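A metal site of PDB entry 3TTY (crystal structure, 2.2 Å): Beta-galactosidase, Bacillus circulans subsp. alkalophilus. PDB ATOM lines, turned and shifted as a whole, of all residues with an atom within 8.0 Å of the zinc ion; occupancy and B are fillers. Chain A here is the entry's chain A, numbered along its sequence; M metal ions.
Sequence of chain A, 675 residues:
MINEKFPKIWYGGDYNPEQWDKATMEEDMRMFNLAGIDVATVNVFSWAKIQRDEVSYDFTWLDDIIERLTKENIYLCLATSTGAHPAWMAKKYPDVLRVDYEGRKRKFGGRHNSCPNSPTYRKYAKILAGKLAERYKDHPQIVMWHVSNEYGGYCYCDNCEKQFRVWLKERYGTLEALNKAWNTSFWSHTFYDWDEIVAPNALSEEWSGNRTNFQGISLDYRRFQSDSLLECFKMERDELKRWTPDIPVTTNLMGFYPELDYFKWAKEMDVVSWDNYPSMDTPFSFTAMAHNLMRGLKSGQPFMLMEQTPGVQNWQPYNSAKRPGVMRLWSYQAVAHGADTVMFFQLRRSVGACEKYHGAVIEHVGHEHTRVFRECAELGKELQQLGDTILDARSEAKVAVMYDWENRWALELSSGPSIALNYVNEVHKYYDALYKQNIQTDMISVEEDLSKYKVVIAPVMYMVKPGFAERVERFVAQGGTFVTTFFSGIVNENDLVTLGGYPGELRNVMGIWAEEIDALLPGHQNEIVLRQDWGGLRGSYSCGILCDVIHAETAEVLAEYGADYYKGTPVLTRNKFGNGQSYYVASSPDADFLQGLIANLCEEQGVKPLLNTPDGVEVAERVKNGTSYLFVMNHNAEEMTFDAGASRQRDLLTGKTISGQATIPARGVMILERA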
ATOM      1  N   ASP A  95       9.572  -9.973  -3.575  1.00  0.00           N
ATOM      2  CA  ASP A  95      10.890  -9.523  -4.092  1.00  0.00           C
ATOM      3  C   ASP A  95      11.498  -8.466  -3.174  1.00  0.00           C
ATOM      4  O   ASP A  95      12.665  -8.135  -3.250  1.00  0.00           O
ATOM      5  CB  ASP A  95      10.777  -8.988  -5.534  1.00  0.00           C
ATOM      6  CG  ASP A  95      10.056  -7.652  -5.610  1.00  0.00           C
ATOM      7  OD1 ASP A  95       8.813  -7.649  -5.728  1.00  0.00           O
ATOM      8  OD2 ASP A  95      10.729  -6.602  -5.547  1.00  0.00           O
ATOM      9  N   VAL A  96      10.677  -7.947  -2.291  1.00  0.00           N
ATOM     10  CA  VAL A  96      11.128  -6.944  -1.342  1.00  0.00           C
ATOM     11  C   VAL A  96      11.943  -7.588  -0.203  1.00  0.00           C
ATOM     12  O   VAL A  96      12.746  -6.941   0.449  1.00  0.00           O
ATOM     13  CB  VAL A  96       9.907  -6.162  -0.836  1.00  0.00           C
ATOM     14  CG1 VAL A  96       9.764  -6.239   0.681  1.00  0.00           C
ATOM     15  CG2 VAL A  96       9.948  -4.740  -1.369  1.00  0.00           C
ATOM     16  N   LEU A  97      11.771  -8.891  -0.035  1.00  0.00           N
ATOM     17  CA  LEU A  97      12.356  -9.614   1.091  1.00  0.00           C
ATOM     18  C   LEU A  97      13.718 -10.219   0.740  1.00  0.00           C
ATOM     19  O   LEU A  97      13.941 -10.701  -0.378  1.00  0.00           O
ATOM     20  CB  LEU A  97      11.409 -10.713   1.555  1.00  0.00           C
ATOM     21  CG  LEU A  97      10.048 -10.288   2.107  1.00  0.00           C
ATOM     22  CD1 LEU A  97       9.112 -11.482   2.155  1.00  0.00           C
ATOM     23  CD2 LEU A  97      10.175  -9.627   3.479  1.00  0.00           C
ATOM     24  N   ARG A  98      14.614 -10.223   1.723  1.00  0.00           N
ATOM     25  CA  ARG A  98      15.972 -10.731   1.501  1.00  0.00           C
ATOM     26  C   ARG A  98      16.069 -12.249   1.577  1.00  0.00           C
ATOM     27  O   ARG A  98      15.167 -12.923   2.094  1.00  0.00           O
ATOM     28  CB  ARG A  98      16.952 -10.094   2.492  1.00  0.00           C
ATOM     29  CG  ARG A  98      17.269  -8.652   2.183  1.00  0.00           C
ATOM     30  CD  ARG A  98      18.258  -8.051   3.138  1.00  0.00           C
ATOM     31  NE  ARG A  98      18.409  -6.621   2.891  1.00  0.00           N
ATOM     32  CZ  ARG A  98      19.108  -5.795   3.664  1.00  0.00           C
ATOM     33  NH1 ARG A  98      19.718  -6.256   4.763  1.00  0.00           N
ATOM     34  NH2 ARG A  98      19.178  -4.514   3.368  1.00  0.00           N
ATOM     35  N   VAL A  99      17.146 -12.776   1.007  1.00  0.00           N
ATOM     36  CA  VAL A  99      17.559 -14.141   1.212  1.00  0.00           C
ATOM     37  C   VAL A  99      18.840 -14.068   2.036  1.00  0.00           C
ATOM     38  O   VAL A  99      19.757 -13.289   1.729  1.00  0.00           O
ATOM     39  CB  VAL A  99      17.757 -14.864  -0.120  1.00  0.00           C
ATOM     40  CG1 VAL A  99      18.584 -16.131   0.046  1.00  0.00           C
ATOM     41  CG2 VAL A  99      16.399 -15.187  -0.710  1.00  0.00           C
ATOM     42  N   LYS A 105      14.950 -17.737   2.176  1.00  0.00           N
ATOM     43  CA  LYS A 105      14.087 -16.598   1.860  1.00  0.00           C
ATOM     44  C   LYS A 105      13.347 -16.087   3.118  1.00  0.00           C
ATOM     45  O   LYS A 105      12.567 -16.809   3.743  1.00  0.00           O
ATOM     46  CB  LYS A 105      13.079 -17.001   0.772  1.00  0.00           C
ATOM     47  CG  LYS A 105      12.104 -15.888   0.380  1.00  0.00           C
ATOM     48  CD  LYS A 105      12.821 -14.727  -0.300  1.00  0.00           C
ATOM     49  CE  LYS A 105      11.837 -13.828  -1.049  1.00  0.00           C
ATOM     50  NZ  LYS A 105      12.484 -12.745  -1.836  1.00  0.00           N
ATOM     51  N   ASN A 113      15.863  -4.385   6.210  1.00  0.00           N
ATOM     52  CA  ASN A 113      16.157  -5.634   5.522  1.00  0.00           C
ATOM     53  C   ASN A 113      15.421  -5.766   4.167  1.00  0.00           C
ATOM     54  O   ASN A 113      15.076  -6.869   3.756  1.00  0.00           O
ATOM     55  CB  ASN A 113      15.827  -6.824   6.445  1.00  0.00           C
ATOM     56  CG  ASN A 113      14.390  -6.782   6.976  1.00  0.00           C
ATOM     57  OD1 ASN A 113      13.573  -5.978   6.494  1.00  0.00           O
ATOM     58  ND2 ASN A 113      14.073  -7.634   7.952  1.00  0.00           N
ATOM     59  N   SER A 114      15.188  -4.655   3.480  1.00  0.00           N
ATOM     60  CA  SER A 114      14.637  -4.721   2.124  1.00  0.00           C
ATOM     61  C   SER A 114      15.738  -5.071   1.127  1.00  0.00           C
ATOM     62  O   SER A 114      16.861  -4.586   1.235  1.00  0.00           O
ATOM     63  CB  SER A 114      13.958  -3.412   1.729  1.00  0.00           C
ATOM     64  OG  SER A 114      12.807  -3.150   2.528  1.00  0.00           O
ATOM     65  N   CYS A 115      15.442  -5.922   0.146  1.00  0.00           N
ATOM     66  CA  CYS A 115      16.474  -6.238  -0.843  1.00  0.00           C
ATOM     67  C   CYS A 115      16.802  -4.954  -1.608  1.00  0.00           C
ATOM     68  O   CYS A 115      15.911  -4.338  -2.197  1.00  0.00           O
ATOM     69  CB  CYS A 115      16.019  -7.342  -1.799  1.00  0.00           C
ATOM     70  SG  CYS A 115      16.999  -7.388  -3.318  1.00  0.00           S
ATOM     71  N   PRO A 116      18.080  -4.561  -1.606  1.00  0.00           N
ATOM     72  CA  PRO A 116      18.477  -3.293  -2.222  1.00  0.00           C
ATOM     73  C   PRO A 116      18.422  -3.372  -3.745  1.00  0.00           C
ATOM     74  O   PRO A 116      18.515  -2.364  -4.418  1.00  0.00           O
ATOM     75  CB  PRO A 116      19.925  -3.114  -1.754  1.00  0.00           C
ATOM     76  CG  PRO A 116      20.413  -4.512  -1.590  1.00  0.00           C
ATOM     77  CD  PRO A 116      19.232  -5.310  -1.092  1.00  0.00           C
ATOM     78  N   ASN A 117      18.258  -4.573  -4.275  1.00  0.00           N
ATOM     79  CA  ASN A 117      18.123  -4.736  -5.712  1.00  0.00           C
ATOM     80  C   ASN A 117      16.694  -5.083  -6.111  1.00  0.00           C
ATOM     81  O   ASN A 117      16.466  -5.640  -7.184  1.00  0.00           O
ATOM     82  CB  ASN A 117      19.105  -5.781  -6.233  1.00  0.00           C
ATOM     83  CG  ASN A 117      20.501  -5.218  -6.392  1.00  0.00           C
ATOM     84  OD1 ASN A 117      20.691  -4.221  -7.094  1.00  0.00           O
ATOM     85  ND2 ASN A 117      21.474  -5.804  -5.697  1.00  0.00           N
ATOM     86  N   SER A 118      15.752  -4.718  -5.260  1.00  0.00           N
ATOM     87  CA  SER A 118      14.337  -5.049  -5.454  1.00  0.00           C
ATOM     88  C   SER A 118      13.591  -3.996  -6.278  1.00  0.00           C
ATOM     89  O   SER A 118      13.577  -2.817  -5.936  1.00  0.00           O
ATOM     90  CB  SER A 118      13.663  -5.250  -4.099  1.00  0.00           C
ATOM     91  OG  SER A 118      12.257  -5.127  -4.211  1.00  0.00           O
ATOM     92  N   TYR A 154      23.505  -7.883   4.308  1.00  0.00           N
ATOM     93  CA  TYR A 154      23.677  -8.335   2.935  1.00  0.00           C
ATOM     94  C   TYR A 154      22.491  -9.186   2.504  1.00  0.00           C
ATOM     95  O   TYR A 154      21.814  -9.778   3.345  1.00  0.00           O
ATOM     96  CB  TYR A 154      24.950  -9.136   2.773  1.00  0.00           C
ATOM     97  CG  TYR A 154      26.195  -8.343   2.982  1.00  0.00           C
ATOM     98  CD1 TYR A 154      26.238  -7.001   2.674  1.00  0.00           C
ATOM     99  CD2 TYR A 154      27.327  -8.934   3.519  1.00  0.00           C
ATOM    100  CE1 TYR A 154      27.381  -6.265   2.866  1.00  0.00           C
ATOM    101  CE2 TYR A 154      28.476  -8.201   3.724  1.00  0.00           C
ATOM    102  CZ  TYR A 154      28.496  -6.864   3.393  1.00  0.00           C
ATOM    103  OH  TYR A 154      29.649  -6.126   3.605  1.00  0.00           O
ATOM    104  N   CYS A 155      22.256  -9.224   1.197  1.00  0.00           N
ATOM    105  CA  CYS A 155      21.225 -10.065   0.613  1.00  0.00           C
ATOM    106  C   CYS A 155      21.873 -10.984  -0.410  1.00  0.00           C
ATOM    107  O   CYS A 155      22.852 -10.604  -1.072  1.00  0.00           O
ATOM    108  CB  CYS A 155      20.159  -9.204  -0.053  1.00  0.00           C
ATOM    109  SG  CYS A 155      18.820 -10.157  -0.814  1.00  0.00           S
ATOM    110  N   TYR A 156      21.319 -12.193  -0.550  1.00  0.00           N
ATOM    111  CA  TYR A 156      21.860 -13.207  -1.447  1.00  0.00           C
ATOM    112  C   TYR A 156      20.783 -13.768  -2.345  1.00  0.00           C
ATOM    113  O   TYR A 156      20.899 -14.903  -2.800  1.00  0.00           O
ATOM    114  CB  TYR A 156      22.514 -14.328  -0.639  1.00  0.00           C
ATOM    115  CG  TYR A 156      23.597 -13.825   0.298  1.00  0.00           C
ATOM    116  CD1 TYR A 156      24.924 -13.706  -0.137  1.00  0.00           C
ATOM    117  CD2 TYR A 156      23.307 -13.442   1.604  1.00  0.00           C
ATOM    118  CE1 TYR A 156      25.922 -13.255   0.698  1.00  0.00           C
ATOM    119  CE2 TYR A 156      24.297 -12.986   2.468  1.00  0.00           C
ATOM    120  CZ  TYR A 156      25.601 -12.893   1.996  1.00  0.00           C
ATOM    121  OH  TYR A 156      26.583 -12.437   2.824  1.00  0.00           O
ATOM    122  N   CYS A 157      19.732 -12.982  -2.601  1.00  0.00           N
ATOM    123  CA  CYS A 157      18.603 -13.456  -3.416  1.00  0.00           C
ATOM    124  C   CYS A 157      18.949 -13.536  -4.910  1.00  0.00           C
ATOM    125  O   CYS A 157      20.038 -13.134  -5.338  1.00  0.00           O
ATOM    126  CB  CYS A 157      17.351 -12.570  -3.204  1.00  0.00           C
ATOM    127  SG  CYS A 157      17.364 -10.990  -4.145  1.00  0.00           S
ATOM    128  N   ASP A 158      18.030 -14.044  -5.699  1.00  0.00           N
ATOM    129  CA  ASP A 158      18.223 -14.116  -7.139  1.00  0.00           C
ATOM    130  C   ASP A 158      18.512 -12.784  -7.842  1.00  0.00           C
ATOM    131  O   ASP A 158      19.346 -12.712  -8.745  1.00  0.00           O
ATOM    132  CB  ASP A 158      17.001 -14.746  -7.792  1.00  0.00           C
ATOM    133  CG  ASP A 158      17.343 -16.025  -8.461  1.00  0.00           C
ATOM    134  OD1 ASP A 158      17.416 -17.057  -7.740  1.00  0.00           O
ATOM    135  OD2 ASP A 158      17.585 -15.988  -9.690  1.00  0.00           O
ATOM    136  N   ASN A 159      17.805 -11.739  -7.434  1.00  0.00           N
ATOM    137  CA  ASN A 159      18.009 -10.424  -8.026  1.00  0.00           C
ATOM    138  C   ASN A 159      19.388  -9.844  -7.722  1.00  0.00           C
ATOM    139  O   ASN A 159      20.027  -9.253  -8.594  1.00  0.00           O
ATOM    140  CB  ASN A 159      16.875  -9.476  -7.628  1.00  0.00           C
ATOM    141  CG  ASN A 159      15.558  -9.847  -8.296  1.00  0.00           C
ATOM    142  OD1 ASN A 159      15.558 -10.454  -9.370  1.00  0.00           O
ATOM    143  ND2 ASN A 159      14.450  -9.518  -7.673  1.00  0.00           N
ATOM    144  N   CYS A 160      19.846 -10.033  -6.482  1.00  0.00           N
ATOM    145  CA  CYS A 160      21.190  -9.596  -6.135  1.00  0.00           C
ATOM    146  C   CYS A 160      22.187 -10.415  -6.915  1.00  0.00           C
ATOM    147  O   CYS A 160      23.175  -9.881  -7.401  1.00  0.00           O
ATOM    148  CB  CYS A 160      21.442  -9.704  -4.633  1.00  0.00           C
ATOM    149  SG  CYS A 160      20.677  -8.371  -3.694  1.00  0.00           S
ATOM    150  N   GLU A 161      21.915 -11.703  -7.071  1.00  0.00           N
ATOM    151  CA  GLU A 161      22.854 -12.584  -7.754  1.00  0.00           C
ATOM    152  C   GLU A 161      23.001 -12.158  -9.219  1.00  0.00           C
ATOM    153  O   GLU A 161      24.120 -11.987  -9.708  1.00  0.00           O
ATOM    154  CB  GLU A 161      22.408 -14.052  -7.648  1.00  0.00           C
ATOM    155  CG  GLU A 161      23.492 -15.047  -7.964  1.00  0.00           C
ATOM    156  CD  GLU A 161      23.186 -16.419  -7.389  1.00  0.00           C
ATOM    157  OE1 GLU A 161      23.950 -16.869  -6.513  1.00  0.00           O
ATOM    158  OE2 GLU A 161      22.182 -17.034  -7.818  1.00  0.00           O
ATOM    159  N   GLN A 163      22.278  -9.250 -10.446  1.00  0.00           N
ATOM    160  CA  GLN A 163      22.822  -7.901 -10.529  1.00  0.00           C
ATOM    161  C   GLN A 163      24.312  -7.920 -10.183  1.00  0.00           C
ATOM    162  O   GLN A 163      25.090  -7.141 -10.723  1.00  0.00           O
ATOM    163  CB  GLN A 163      22.005  -6.944  -9.659  1.00  0.00           C
ATOM    164  CG  GLN A 163      22.372  -5.485  -9.804  1.00  0.00           C
ATOM    165  CD  GLN A 163      22.314  -4.979 -11.261  1.00  0.00           C
ATOM    166  OE1 GLN A 163      21.507  -5.435 -12.079  1.00  0.00           O
ATOM    167  NE2 GLN A 163      23.186  -4.018 -11.560  1.00  0.00           N
ATOM    168  N   TYR A 221      31.756  -9.138  -3.637  1.00  0.00           N
ATOM    169  CA  TYR A 221      30.335  -9.172  -3.314  1.00  0.00           C
ATOM    170  C   TYR A 221      30.009  -8.131  -2.228  1.00  0.00           C
ATOM    171  O   TYR A 221      28.964  -7.452  -2.283  1.00  0.00           O
ATOM    172  CB  TYR A 221      29.885 -10.572  -2.904  1.00  0.00           C
ATOM    173  CG  TYR A 221      28.401 -10.740  -2.990  1.00  0.00           C
ATOM    174  CD1 TYR A 221      27.772 -10.953  -4.229  1.00  0.00           C
ATOM    175  CD2 TYR A 221      27.605 -10.681  -1.842  1.00  0.00           C
ATOM    176  CE1 TYR A 221      26.387 -11.106  -4.307  1.00  0.00           C
ATOM    177  CE2 TYR A 221      26.233 -10.831  -1.917  1.00  0.00           C
ATOM    178  CZ  TYR A 221      25.631 -11.038  -3.151  1.00  0.00           C
ATOM    179  OH  TYR A 221      24.277 -11.171  -3.222  1.00  0.00           O
ATOM    180  N   PHE A 224      29.834  -4.871  -3.823  1.00  0.00           N
ATOM    181  CA  PHE A 224      28.597  -4.839  -4.586  1.00  0.00           C
ATOM    182  C   PHE A 224      27.379  -4.545  -3.709  1.00  0.00           C
ATOM    183  O   PHE A 224      26.557  -3.657  -4.010  1.00  0.00           O
ATOM    184  CB  PHE A 224      28.433  -6.171  -5.330  1.00  0.00           C
ATOM    185  CG  PHE A 224      27.051  -6.438  -5.833  1.00  0.00           C
ATOM    186  CD1 PHE A 224      26.477  -5.618  -6.797  1.00  0.00           C
ATOM    187  CD2 PHE A 224      26.319  -7.511  -5.361  1.00  0.00           C
ATOM    188  CE1 PHE A 224      25.194  -5.858  -7.273  1.00  0.00           C
ATOM    189  CE2 PHE A 224      25.032  -7.752  -5.821  1.00  0.00           C
ATOM    190  CZ  PHE A 224      24.467  -6.913  -6.776  1.00  0.00           C
ATOM    191  N   GLN A 225      27.258  -5.298  -2.614  1.00  0.00           N
ATOM    192  CA  GLN A 225      26.180  -5.085  -1.645  1.00  0.00           C
ATOM    193  C   GLN A 225      26.213  -3.655  -1.096  1.00  0.00           C
ATOM    194  O   GLN A 225      25.192  -2.977  -1.012  1.00  0.00           O
ATOM    195  CB  GLN A 225      26.287  -6.107  -0.517  1.00  0.00           C
ATOM    196  CG  GLN A 225      25.756  -7.499  -0.916  1.00  0.00           C
ATOM    197  CD  GLN A 225      24.278  -7.474  -1.219  1.00  0.00           C
ATOM    198  OE1 GLN A 225      23.458  -7.290  -0.315  1.00  0.00           O
ATOM    199  NE2 GLN A 225      23.918  -7.643  -2.487  1.00  0.00           N
ATOM    200  N   SER A 228      25.065  -1.360  -3.814  1.00  0.00           N
ATOM    201  CA  SER A 228      23.627  -1.514  -4.066  1.00  0.00           C
ATOM    202  C   SER A 228      22.779  -0.735  -3.060  1.00  0.00           C
ATOM    203  O   SER A 228      21.808  -0.071  -3.421  1.00  0.00           O
ATOM    204  CB  SER A 228      23.217  -2.985  -4.024  1.00  0.00           C
ATOM    205  OG  SER A 228      23.874  -3.765  -5.002  1.00  0.00           O
HETATM  206 ZN    ZN M   1      18.642  -9.164  -2.970  1.00  0.00          ZN
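SG of Cys 160 lies close to NE2 of Gln 225 (3.5 Å). The side-chain sulfur of Cys 157 sits close to the backbone NH of Asn 159 (3.4 Å). The backbone NH (N) of Cys 115 lies within hydrogen-bond range of the backbone carbonyl oxygen (O) of Val 96. O of Cys 155 is in hydrogen-bond range of OH of Tyr 221 (2.6 Å). The side-chain sulfur (SG) of Cys 155 sits close to the backbone NH (N) of Val 99 (3.6 Å). The side-chain sulfur (SG) of Cys 115 lies close to the backbone NH (N) of Ser 118 (3.5 Å). N of Asn 117 sits close to SG of Cys 115. The side-chain sulfur (SG) of Cys 160 lies close to the side-chain amide nitrogen (ND2) of Asn 117, 3.4 Å away.
The zinc ion is bound by SG of Cys 160 (2.3 Å), SG of Cys 155 (2.4 Å), SG of Cys 115 (2.4 Å) and SG of Cys 157 (2.5 Å).
Within 4 Å of the zinc ion: Cys 115, Cys 155, Cys 157 and Cys 160. The nearest printed residue that does not touch the zinc ion is Pro 116 (4.3 Å).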
